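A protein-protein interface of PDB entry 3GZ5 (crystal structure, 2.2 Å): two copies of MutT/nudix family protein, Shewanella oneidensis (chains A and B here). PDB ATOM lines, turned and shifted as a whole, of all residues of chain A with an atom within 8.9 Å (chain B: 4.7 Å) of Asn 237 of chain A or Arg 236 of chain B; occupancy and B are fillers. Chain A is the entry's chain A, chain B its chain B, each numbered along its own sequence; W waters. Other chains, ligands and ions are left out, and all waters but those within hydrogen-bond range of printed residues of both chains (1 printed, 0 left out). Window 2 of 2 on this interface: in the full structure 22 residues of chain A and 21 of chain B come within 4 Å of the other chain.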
ATOM      1  N   THR A 157     -23.176 -35.414  10.586  1.00  0.00           N
ATOM      2  CA  THR A 157     -24.095 -34.752  11.518  1.00  0.00           C
ATOM      3  C   THR A 157     -23.488 -33.452  12.071  1.00  0.00           C
ATOM      4  O   THR A 157     -24.134 -32.412  12.048  1.00  0.00           O
ATOM      5  CB  THR A 157     -24.590 -35.738  12.611  1.00  0.00           C
ATOM      6  OG1 THR A 157     -25.447 -36.688  11.972  1.00  0.00           O
ATOM      7  CG2 THR A 157     -25.343 -35.033  13.731  1.00  0.00           C
ATOM      8  N   GLN A 158     -22.240 -33.522  12.516  1.00  0.00           N
ATOM      9  CA  GLN A 158     -21.470 -32.335  12.878  1.00  0.00           C
ATOM     10  C   GLN A 158     -21.392 -31.280  11.761  1.00  0.00           C
ATOM     11  O   GLN A 158     -21.557 -30.103  12.020  1.00  0.00           O
ATOM     12  CB  GLN A 158     -20.063 -32.747  13.282  1.00  0.00           C
ATOM     13  CG  GLN A 158     -20.047 -33.680  14.458  1.00  0.00           C
ATOM     14  CD  GLN A 158     -20.527 -32.974  15.693  1.00  0.00           C
ATOM     15  OE1 GLN A 158     -19.971 -31.924  16.070  1.00  0.00           O
ATOM     16  NE2 GLN A 158     -21.589 -33.513  16.319  1.00  0.00           N
ATOM     17  N   LYS A 159     -21.129 -31.696  10.525  1.00  0.00           N
ATOM     18  CA  LYS A 159     -21.157 -30.777   9.373  1.00  0.00           C
ATOM     19  C   LYS A 159     -22.481 -30.030   9.260  1.00  0.00           C
ATOM     20  O   LYS A 159     -22.524 -28.850   8.876  1.00  0.00           O
ATOM     21  CB  LYS A 159     -20.885 -31.533   8.058  1.00  0.00           C
ATOM     22  CG  LYS A 159     -19.499 -32.181   7.959  1.00  0.00           C
ATOM     23  CD  LYS A 159     -18.413 -31.178   8.307  1.00  0.00           C
ATOM     24  CE  LYS A 159     -17.058 -31.774   8.108  1.00  0.00           C
ATOM     25  NZ  LYS A 159     -15.997 -30.721   8.272  1.00  0.00           N
ATOM     26  N   ALA A 160     -23.564 -30.736   9.556  1.00  0.00           N
ATOM     27  CA  ALA A 160     -24.890 -30.142   9.547  1.00  0.00           C
ATOM     28  C   ALA A 160     -25.034 -29.146  10.697  1.00  0.00           C
ATOM     29  O   ALA A 160     -25.726 -28.154  10.562  1.00  0.00           O
ATOM     30  CB  ALA A 160     -25.965 -31.206   9.612  1.00  0.00           C
ATOM     31  N   LEU A 161     -24.345 -29.383  11.802  1.00  0.00           N
ATOM     32  CA  LEU A 161     -24.397 -28.457  12.923  1.00  0.00           C
ATOM     33  C   LEU A 161     -23.562 -27.177  12.715  1.00  0.00           C
ATOM     34  O   LEU A 161     -23.952 -26.117  13.209  1.00  0.00           O
ATOM     35  CB  LEU A 161     -24.027 -29.160  14.258  1.00  0.00           C
ATOM     36  CG  LEU A 161     -25.051 -30.136  14.874  1.00  0.00           C
ATOM     37  CD1 LEU A 161     -24.469 -30.946  16.023  1.00  0.00           C
ATOM     38  CD2 LEU A 161     -26.321 -29.426  15.359  1.00  0.00           C
ATOM     39  N   TYR A 162     -22.424 -27.275  12.012  1.00  0.00           N
ATOM     40  CA  TYR A 162     -21.412 -26.206  12.010  1.00  0.00           C
ATOM     41  C   TYR A 162     -20.961 -25.638  10.647  1.00  0.00           C
ATOM     42  O   TYR A 162     -20.060 -24.818  10.596  1.00  0.00           O
ATOM     43  CB  TYR A 162     -20.170 -26.657  12.793  1.00  0.00           C
ATOM     44  CG  TYR A 162     -20.462 -26.871  14.255  1.00  0.00           C
ATOM     45  CD1 TYR A 162     -20.572 -28.167  14.774  1.00  0.00           C
ATOM     46  CD2 TYR A 162     -20.673 -25.788  15.113  1.00  0.00           C
ATOM     47  CE1 TYR A 162     -20.874 -28.385  16.110  1.00  0.00           C
ATOM     48  CE2 TYR A 162     -20.962 -25.999  16.473  1.00  0.00           C
ATOM     49  CZ  TYR A 162     -21.074 -27.302  16.957  1.00  0.00           C
ATOM     50  OH  TYR A 162     -21.379 -27.548  18.285  1.00  0.00           O
ATOM     51  N   SER A 163     -21.581 -26.067   9.557  1.00  0.00           N
ATOM     52  CA  SER A 163     -21.095 -25.705   8.225  1.00  0.00           C
ATOM     53  C   SER A 163     -22.244 -25.789   7.239  1.00  0.00           C
ATOM     54  O   SER A 163     -23.340 -26.242   7.605  1.00  0.00           O
ATOM     55  CB  SER A 163     -19.995 -26.689   7.796  1.00  0.00           C
ATOM     56  OG  SER A 163     -20.575 -27.909   7.362  1.00  0.00           O
ATOM     57  N   LEU A 187     -29.555 -34.129  10.551  1.00  0.00           N
ATOM     58  CA  LEU A 187     -29.785 -33.854  11.971  1.00  0.00           C
ATOM     59  C   LEU A 187     -30.833 -34.789  12.587  1.00  0.00           C
ATOM     60  O   LEU A 187     -30.790 -35.050  13.787  1.00  0.00           O
ATOM     61  CB  LEU A 187     -30.132 -32.378  12.209  1.00  0.00           C
ATOM     62  CG  LEU A 187     -28.976 -31.392  11.965  1.00  0.00           C
ATOM     63  CD1 LEU A 187     -29.401 -29.908  12.132  1.00  0.00           C
ATOM     64  CD2 LEU A 187     -27.750 -31.727  12.843  1.00  0.00           C
ATOM     65  N   LYS A 189     -34.214 -34.235  12.472  1.00  0.00           N
ATOM     66  CA  LYS A 189     -35.257 -33.406  13.070  1.00  0.00           C
ATOM     67  C   LYS A 189     -35.437 -32.123  12.274  1.00  0.00           C
ATOM     68  O   LYS A 189     -34.484 -31.664  11.638  1.00  0.00           O
ATOM     69  CB  LYS A 189     -34.951 -33.090  14.550  1.00  0.00           C
ATOM     70  CG  LYS A 189     -33.618 -32.447  14.839  1.00  0.00           C
ATOM     71  CD  LYS A 189     -33.205 -32.802  16.244  1.00  0.00           C
ATOM     72  CE  LYS A 189     -31.998 -32.027  16.703  1.00  0.00           C
ATOM     73  NZ  LYS A 189     -31.319 -32.773  17.802  1.00  0.00           N
ATOM     74  N   ILE A 191     -36.016 -28.032  11.496  1.00  0.00           N
ATOM     75  CA  ILE A 191     -35.172 -26.914  11.870  1.00  0.00           C
ATOM     76  C   ILE A 191     -35.936 -25.617  11.573  1.00  0.00           C
ATOM     77  O   ILE A 191     -36.693 -25.545  10.598  1.00  0.00           O
ATOM     78  CB  ILE A 191     -33.784 -26.997  11.130  1.00  0.00           C
ATOM     79  CG1 ILE A 191     -32.785 -25.988  11.675  1.00  0.00           C
ATOM     80  CG2 ILE A 191     -33.926 -26.800   9.636  1.00  0.00           C
ATOM     81  CD1 ILE A 191     -31.798 -25.565  10.643  1.00  0.00           C
ATOM     82  N   SER A 195     -34.216 -18.960  11.391  1.00  0.00           N
ATOM     83  CA  SER A 195     -32.874 -18.901  11.957  1.00  0.00           C
ATOM     84  C   SER A 195     -31.818 -19.538  11.030  1.00  0.00           C
ATOM     85  O   SER A 195     -30.673 -19.109  11.049  1.00  0.00           O
ATOM     86  CB  SER A 195     -32.837 -19.519  13.360  1.00  0.00           C
ATOM     87  OG  SER A 195     -33.103 -20.910  13.327  1.00  0.00           O
ATOM     88  N   ARG A 198     -31.250 -16.971   8.133  1.00  0.00           N
ATOM     89  CA  ARG A 198     -30.424 -15.954   8.783  1.00  0.00           C
ATOM     90  C   ARG A 198     -28.940 -16.359   8.839  1.00  0.00           C
ATOM     91  O   ARG A 198     -28.049 -15.577   8.470  1.00  0.00           O
ATOM     92  CB  ARG A 198     -30.914 -15.727  10.213  1.00  0.00           C
ATOM     93  CG  ARG A 198     -30.195 -14.599  10.927  1.00  0.00           C
ATOM     94  CD  ARG A 198     -30.001 -14.899  12.404  1.00  0.00           C
ATOM     95  NE  ARG A 198     -29.333 -13.789  13.080  1.00  0.00           N
ATOM     96  CZ  ARG A 198     -28.896 -13.821  14.340  1.00  0.00           C
ATOM     97  NH1 ARG A 198     -28.300 -12.748  14.862  1.00  0.00           N
ATOM     98  NH2 ARG A 198     -29.039 -14.925  15.078  1.00  0.00           N
ATOM     99  N   ARG A 199     -28.715 -17.566   9.358  1.00  0.00           N
ATOM    100  CA  ARG A 199     -27.412 -18.232   9.446  1.00  0.00           C
ATOM    101  C   ARG A 199     -26.698 -18.266   8.081  1.00  0.00           C
ATOM    102  O   ARG A 199     -25.566 -17.799   7.952  1.00  0.00           O
ATOM    103  CB  ARG A 199     -27.662 -19.648   9.962  1.00  0.00           C
ATOM    104  CG  ARG A 199     -26.479 -20.519  10.229  1.00  0.00           C
ATOM    105  CD  ARG A 199     -26.998 -21.742  10.969  1.00  0.00           C
ATOM    106  NE  ARG A 199     -26.035 -22.836  11.090  1.00  0.00           N
ATOM    107  CZ  ARG A 199     -25.053 -22.881  11.989  1.00  0.00           C
ATOM    108  NH1 ARG A 199     -24.878 -21.873  12.849  1.00  0.00           N
ATOM    109  NH2 ARG A 199     -24.244 -23.934  12.026  1.00  0.00           N
ATOM    110  N   ARG A 233     -16.596 -22.556   8.915  1.00  0.00           N
ATOM    111  CA  ARG A 233     -17.311 -23.158  10.063  1.00  0.00           C
ATOM    112  C   ARG A 233     -18.044 -22.091  10.855  1.00  0.00           C
ATOM    113  O   ARG A 233     -17.502 -20.999  11.068  1.00  0.00           O
ATOM    114  CB  ARG A 233     -16.347 -23.896  10.998  1.00  0.00           C
ATOM    115  CG  ARG A 233     -15.587 -25.074  10.359  1.00  0.00           C
ATOM    116  CD  ARG A 233     -16.545 -26.054   9.657  1.00  0.00           C
ATOM    117  NE  ARG A 233     -15.868 -27.110   8.889  1.00  0.00           N
ATOM    118  CZ  ARG A 233     -15.815 -27.163   7.559  1.00  0.00           C
ATOM    119  NH1 ARG A 233     -16.383 -26.218   6.829  1.00  0.00           N
ATOM    120  NH2 ARG A 233     -15.179 -28.162   6.953  1.00  0.00           N
ATOM    121  N   PHE A 234     -19.271 -22.403  11.282  1.00  0.00           N
ATOM    122  CA  PHE A 234     -20.025 -21.541  12.199  1.00  0.00           C
ATOM    123  C   PHE A 234     -19.504 -21.761  13.613  1.00  0.00           C
ATOM    124  O   PHE A 234     -19.169 -22.896  13.972  1.00  0.00           O
ATOM    125  CB  PHE A 234     -21.521 -21.857  12.144  1.00  0.00           C
ATOM    126  CG  PHE A 234     -22.167 -21.496  10.836  1.00  0.00           C
ATOM    127  CD1 PHE A 234     -22.731 -20.228  10.645  1.00  0.00           C
ATOM    128  CD2 PHE A 234     -22.210 -22.420   9.787  1.00  0.00           C
ATOM    129  CE1 PHE A 234     -23.336 -19.885   9.424  1.00  0.00           C
ATOM    130  CE2 PHE A 234     -22.802 -22.091   8.569  1.00  0.00           C
ATOM    131  CZ  PHE A 234     -23.371 -20.816   8.386  1.00  0.00           C
ATOM    132  N   LEU A 235     -19.431 -20.687  14.400  1.00  0.00           N
ATOM    133  CA  LEU A 235     -19.022 -20.775  15.808  1.00  0.00           C
ATOM    134  C   LEU A 235     -20.137 -21.391  16.669  1.00  0.00           C
ATOM    135  O   LEU A 235     -19.892 -22.242  17.528  1.00  0.00           O
ATOM    136  CB  LEU A 235     -18.578 -19.406  16.351  1.00  0.00           C
ATOM    137  CG  LEU A 235     -17.069 -19.061  16.327  1.00  0.00           C
ATOM    138  CD1 LEU A 235     -16.522 -18.836  14.924  1.00  0.00           C
ATOM    139  CD2 LEU A 235     -16.735 -17.852  17.201  1.00  0.00           C
ATOM    140  N   ARG A 236     -21.372 -20.978  16.400  1.00  0.00           N
ATOM    141  CA  ARG A 236     -22.514 -21.519  17.115  1.00  0.00           C
ATOM    142  C   ARG A 236     -23.106 -22.662  16.321  1.00  0.00           C
ATOM    143  O   ARG A 236     -23.173 -22.599  15.093  1.00  0.00           O
ATOM    144  CB  ARG A 236     -23.577 -20.440  17.314  1.00  0.00           C
ATOM    145  CG  ARG A 236     -24.270 -20.491  18.670  1.00  0.00           C
ATOM    146  CD  ARG A 236     -24.500 -19.063  19.246  1.00  0.00           C
ATOM    147  NE  ARG A 236     -23.254 -18.288  19.302  1.00  0.00           N
ATOM    148  CZ  ARG A 236     -22.883 -17.390  18.387  1.00  0.00           C
ATOM    149  NH1 ARG A 236     -23.668 -17.142  17.341  1.00  0.00           N
ATOM    150  NH2 ARG A 236     -21.729 -16.734  18.517  1.00  0.00           N
ATOM    151  N   ASN A 237     -23.538 -23.698  17.026  1.00  0.00           N
ATOM    152  CA  ASN A 237     -24.292 -24.764  16.413  1.00  0.00           C
ATOM    153  C   ASN A 237     -25.576 -24.217  15.804  1.00  0.00           C
ATOM    154  O   ASN A 237     -26.065 -23.140  16.175  1.00  0.00           O
ATOM    155  CB  ASN A 237     -24.629 -25.852  17.440  1.00  0.00           C
ATOM    156  CG  ASN A 237     -25.803 -25.471  18.340  1.00  0.00           C
ATOM    157  OD1 ASN A 237     -26.956 -25.829  18.063  1.00  0.00           O
ATOM    158  ND2 ASN A 237     -25.518 -24.732  19.409  1.00  0.00           N
ATOM    159  N   LEU A 238     -26.128 -24.987  14.878  1.00  0.00           N
ATOM    160  CA  LEU A 238     -27.422 -24.689  14.316  1.00  0.00           C
ATOM    161  C   LEU A 238     -28.569 -24.981  15.317  1.00  0.00           C
ATOM    162  O   LEU A 238     -28.912 -26.139  15.601  1.00  0.00           O
ATOM    163  CB  LEU A 238     -27.574 -25.466  13.020  1.00  0.00           C
ATOM    164  CG  LEU A 238     -28.801 -25.230  12.172  1.00  0.00           C
ATOM    165  CD1 LEU A 238     -29.267 -23.772  12.256  1.00  0.00           C
ATOM    166  CD2 LEU A 238     -28.494 -25.672  10.730  1.00  0.00           C
ATOM    167  N   LEU B 161     -12.519 -24.374  22.898  1.00  0.00           N
ATOM    168  CA  LEU B 161     -13.772 -23.702  22.550  1.00  0.00           C
ATOM    169  C   LEU B 161     -15.013 -24.548  22.794  1.00  0.00           C
ATOM    170  O   LEU B 161     -16.104 -24.018  23.094  1.00  0.00           O
ATOM    171  CB  LEU B 161     -13.740 -23.271  21.078  1.00  0.00           C
ATOM    172  CG  LEU B 161     -13.121 -21.920  20.672  1.00  0.00           C
ATOM    173  CD1 LEU B 161     -13.440 -21.666  19.205  1.00  0.00           C
ATOM    174  CD2 LEU B 161     -13.632 -20.731  21.512  1.00  0.00           C
ATOM    175  N   TYR B 162     -14.859 -25.861  22.644  1.00  0.00           N
ATOM    176  CA  TYR B 162     -16.017 -26.755  22.652  1.00  0.00           C
ATOM    177  C   TYR B 162     -15.969 -27.881  23.668  1.00  0.00           C
ATOM    178  O   TYR B 162     -16.855 -28.720  23.658  1.00  0.00           O
ATOM    179  CB  TYR B 162     -16.260 -27.356  21.258  1.00  0.00           C
ATOM    180  CG  TYR B 162     -16.599 -26.336  20.212  1.00  0.00           C
ATOM    181  CD1 TYR B 162     -17.872 -25.761  20.148  1.00  0.00           C
ATOM    182  CD2 TYR B 162     -15.639 -25.929  19.288  1.00  0.00           C
ATOM    183  CE1 TYR B 162     -18.182 -24.800  19.174  1.00  0.00           C
ATOM    184  CE2 TYR B 162     -15.934 -24.975  18.314  1.00  0.00           C
ATOM    185  CZ  TYR B 162     -17.202 -24.426  18.264  1.00  0.00           C
ATOM    186  OH  TYR B 162     -17.460 -23.497  17.293  1.00  0.00           O
ATOM    187  N   ARG B 199     -20.767 -22.455  32.273  1.00  0.00           N
ATOM    188  CA  ARG B 199     -20.694 -23.572  31.310  1.00  0.00           C
ATOM    189  C   ARG B 199     -20.136 -24.861  31.940  1.00  0.00           C
ATOM    190  O   ARG B 199     -20.686 -25.946  31.728  1.00  0.00           O
ATOM    191  CB  ARG B 199     -19.936 -23.170  30.035  1.00  0.00           C
ATOM    192  CG  ARG B 199     -20.861 -22.752  28.861  1.00  0.00           C
ATOM    193  CD  ARG B 199     -20.130 -21.931  27.776  1.00  0.00           C
ATOM    194  NE  ARG B 199     -19.537 -22.752  26.708  1.00  0.00           N
ATOM    195  CZ  ARG B 199     -18.316 -23.296  26.748  1.00  0.00           C
ATOM    196  NH1 ARG B 199     -17.524 -23.126  27.807  1.00  0.00           N
ATOM    197  NH2 ARG B 199     -17.882 -24.016  25.724  1.00  0.00           N
ATOM    198  N   TYR B 232     -17.239 -35.509  25.905  1.00  0.00           N
ATOM    199  CA  TYR B 232     -18.244 -34.433  25.999  1.00  0.00           C
ATOM    200  C   TYR B 232     -17.879 -33.180  25.200  1.00  0.00           C
ATOM    201  O   TYR B 232     -16.781 -32.624  25.362  1.00  0.00           O
ATOM    202  CB  TYR B 232     -18.515 -34.038  27.453  1.00  0.00           C
ATOM    203  CG  TYR B 232     -19.620 -33.001  27.586  1.00  0.00           C
ATOM    204  CD1 TYR B 232     -20.913 -33.376  27.987  1.00  0.00           C
ATOM    205  CD2 TYR B 232     -19.378 -31.647  27.297  1.00  0.00           C
ATOM    206  CE1 TYR B 232     -21.932 -32.434  28.101  1.00  0.00           C
ATOM    207  CE2 TYR B 232     -20.385 -30.694  27.409  1.00  0.00           C
ATOM    208  CZ  TYR B 232     -21.661 -31.091  27.807  1.00  0.00           C
ATOM    209  OH  TYR B 232     -22.654 -30.144  27.911  1.00  0.00           O
ATOM    210  N   PHE B 234     -19.569 -29.256  24.183  1.00  0.00           N
ATOM    211  CA  PHE B 234     -20.588 -28.206  24.209  1.00  0.00           C
ATOM    212  C   PHE B 234     -21.014 -27.933  22.779  1.00  0.00           C
ATOM    213  O   PHE B 234     -20.190 -27.973  21.859  1.00  0.00           O
ATOM    214  CB  PHE B 234     -20.048 -26.888  24.782  1.00  0.00           C
ATOM    215  CG  PHE B 234     -19.603 -26.967  26.211  1.00  0.00           C
ATOM    216  CD1 PHE B 234     -20.530 -26.904  27.247  1.00  0.00           C
ATOM    217  CD2 PHE B 234     -18.249 -27.066  26.526  1.00  0.00           C
ATOM    218  CE1 PHE B 234     -20.114 -26.953  28.573  1.00  0.00           C
ATOM    219  CE2 PHE B 234     -17.821 -27.112  27.845  1.00  0.00           C
ATOM    220  CZ  PHE B 234     -18.753 -27.065  28.872  1.00  0.00           C
ATOM    221  N   LEU B 235     -22.296 -27.649  22.595  1.00  0.00           N
ATOM    222  CA  LEU B 235     -22.819 -27.256  21.283  1.00  0.00           C
ATOM    223  C   LEU B 235     -22.438 -25.812  20.902  1.00  0.00           C
ATOM    224  O   LEU B 235     -22.076 -25.523  19.751  1.00  0.00           O
ATOM    225  CB  LEU B 235     -24.331 -27.502  21.223  1.00  0.00           C
ATOM    226  CG  LEU B 235     -24.767 -28.764  20.460  1.00  0.00           C
ATOM    227  CD1 LEU B 235     -24.186 -30.042  21.072  1.00  0.00           C
ATOM    228  CD2 LEU B 235     -26.298 -28.859  20.357  1.00  0.00           C
ATOM    229  N   ARG B 236     -22.501 -24.911  21.875  1.00  0.00           N
ATOM    230  CA  ARG B 236     -22.080 -23.532  21.682  1.00  0.00           C
ATOM    231  C   ARG B 236     -20.619 -23.349  22.087  1.00  0.00           C
ATOM    232  O   ARG B 236     -20.157 -23.957  23.067  1.00  0.00           O
ATOM    233  CB  ARG B 236     -22.990 -22.542  22.449  1.00  0.00           C
ATOM    234  CG  ARG B 236     -23.926 -23.133  23.560  1.00  0.00           C
ATOM    235  CD  ARG B 236     -23.189 -23.773  24.789  1.00  0.00           C
ATOM    236  NE  ARG B 236     -23.110 -25.245  24.721  1.00  0.00           N
ATOM    237  CZ  ARG B 236     -24.059 -26.088  25.137  1.00  0.00           C
ATOM    238  NH1 ARG B 236     -25.193 -25.635  25.657  1.00  0.00           N
ATOM    239  NH2 ARG B 236     -23.884 -27.397  25.031  1.00  0.00           N
ATOM    240  N   ASN B 237     -19.904 -22.518  21.319  1.00  0.00           N
ATOM    241  CA  ASN B 237     -18.529 -22.115  21.640  1.00  0.00           C
ATOM    242  C   ASN B 237     -18.408 -21.387  22.978  1.00  0.00           C
ATOM    243  O   ASN B 237     -19.398 -20.882  23.517  1.00  0.00           O
ATOM    244  CB  ASN B 237     -17.938 -21.242  20.525  1.00  0.00           C
ATOM    245  CG  ASN B 237     -18.852 -20.076  20.136  1.00  0.00           C
ATOM    246  OD1 ASN B 237     -20.037 -20.264  19.839  1.00  0.00           O
ATOM    247  ND2 ASN B 237     -18.293 -18.867  20.115  1.00  0.00           N
ATOM    248  N   LEU B 238     -17.185 -21.334  23.500  1.00  0.00           N
ATOM    249  CA  LEU B 238     -16.885 -20.670  24.768  1.00  0.00           C
ATOM    250  C   LEU B 238     -17.020 -19.138  24.663  1.00  0.00           C
ATOM    251  O   LEU B 238     -16.270 -18.478  23.927  1.00  0.00           O
ATOM    252  CB  LEU B 238     -15.471 -21.058  25.207  1.00  0.00           C
ATOM    253  CG  LEU B 238     -14.908 -20.675  26.576  1.00  0.00           C
ATOM    254  CD1 LEU B 238     -13.572 -21.387  26.768  1.00  0.00           C
ATOM    255  CD2 LEU B 238     -14.758 -19.163  26.746  1.00  0.00           C
HETATM  256  O   HOH W   1     -20.240 -29.595  19.418  1.00  0.00           O
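The side-chain hydroxyl of Tyr 162 of chain A lies within hydrogen-bond range of the backbone carbonyl oxygen of Leu 235 of chain B (2.6 Å).
The backbone carbonyl oxygen (O) of Leu 235 of chain A lies within hydrogen-bond range of the side-chain hydroxyl (OH) of Tyr 162 of chain B (2.7 Å).
The side-chain amide oxygen (OD1) of Asn 237 of chain B lies close to the backbone carbonyl oxygen (O) of Leu 235 of chain A.
The backbone carbonyl oxygen (O) of Tyr 162 of chain A is in hydrogen-bond range of the backbone NH (N) of Phe 234 of chain A, 2.6 Å away.
NH1 of Arg 199 of chain A sits at hydrogen-bond distance from O of Arg 236 of chain A.
N of Phe 234 of chain B lies within hydrogen-bond range of O of Tyr 162 of chain B (2.8 Å).
NH2 of Arg 199 of chain B sits at hydrogen-bond distance from O of Arg 236 of chain B (3.5 Å).
Among the printed residues, merely in contact across the chains: Asn 237 of chain A with Leu 235 of chain B (3.5 Å), Arg 236 of chain A with Asn 237 of chain B (3.8 Å), Phe 234 of chain A with Tyr 162 of chain B (3.8 Å), Tyr 162 of chain A with Phe 234 of chain B (3.8 Å) and Asn 237 of chain A with Arg 236 of chain B (3.9 Å).
Asn 237 of chain A touches two residues of chain B.
Of chain A, only Asn 237 (3.9 Å) comes within 4 Å of Arg 236 of chain B.
Leu 235 of chain B touches two residues of chain A.
Of the printed residues of chain B, Tyr 162 of chain A touches Phe 234 and Leu 235.
Printed residues of chain B within 4 Å of Leu 235 of chain A: Tyr 162 and Asn 237.
Of the printed residues of chain B, Phe 234 of chain A touches Tyr 162 (3.8 Å).
Of the printed residues of chain A, Phe 234 of chain B touches Tyr 162.
Of the printed residues of chain A, Tyr 162 of chain B touches Phe 234 and Leu 235.
Gln 158 of chain A touches none of the printed residues of chain B.
Leu 161 of chain B touches none of the printed residues of chain A.
The nearest printed residue of chain B that does not touch Asn 237 of chain A is Asn 237 of chain B (5.7 Å).
Along chain A the printed residues that touch a printed residue of chain B span positions 162 to 237.
Hydrophobic or aromatic side chains of chain B that line the printed part of chain A: Tyr 162 and Leu 235.
Among the printed residues, 8 pairs touch across the chains.
Among the printed residues, no Asp or Glu carboxylate lies within 4 Å of a Lys or Arg side-chain nitrogen of the other chain.
Tyr 162 of chain A touches Phe 234 of chain B, and with the chains exchanged Phe 234 of chain A touches Tyr 162 of chain B.
Tyr 162 of chain A touches Leu 235 of chain B, and with the chains exchanged Leu 235 of chain A touches Tyr 162 of chain B.
Leu 235 of chain A touches Asn 237 of chain B, and with the chains exchanged Asn 237 of chain A touches Leu 235 of chain B.
Arg 236 of chain A touches Asn 237 of chain B, and with the chains exchanged Asn 237 of chain A touches Arg 236 of chain B.
Of the 8 pairs that touch across the chains among the printed residues, 8 have their exchanged pair printed and touching as well.
Water W1 lies within hydrogen-bond range of the side-chain hydroxyl of Tyr 162 of chain A (2.6 Å) and the backbone carbonyl oxygen of Phe 234 of chain B (2.9 Å).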
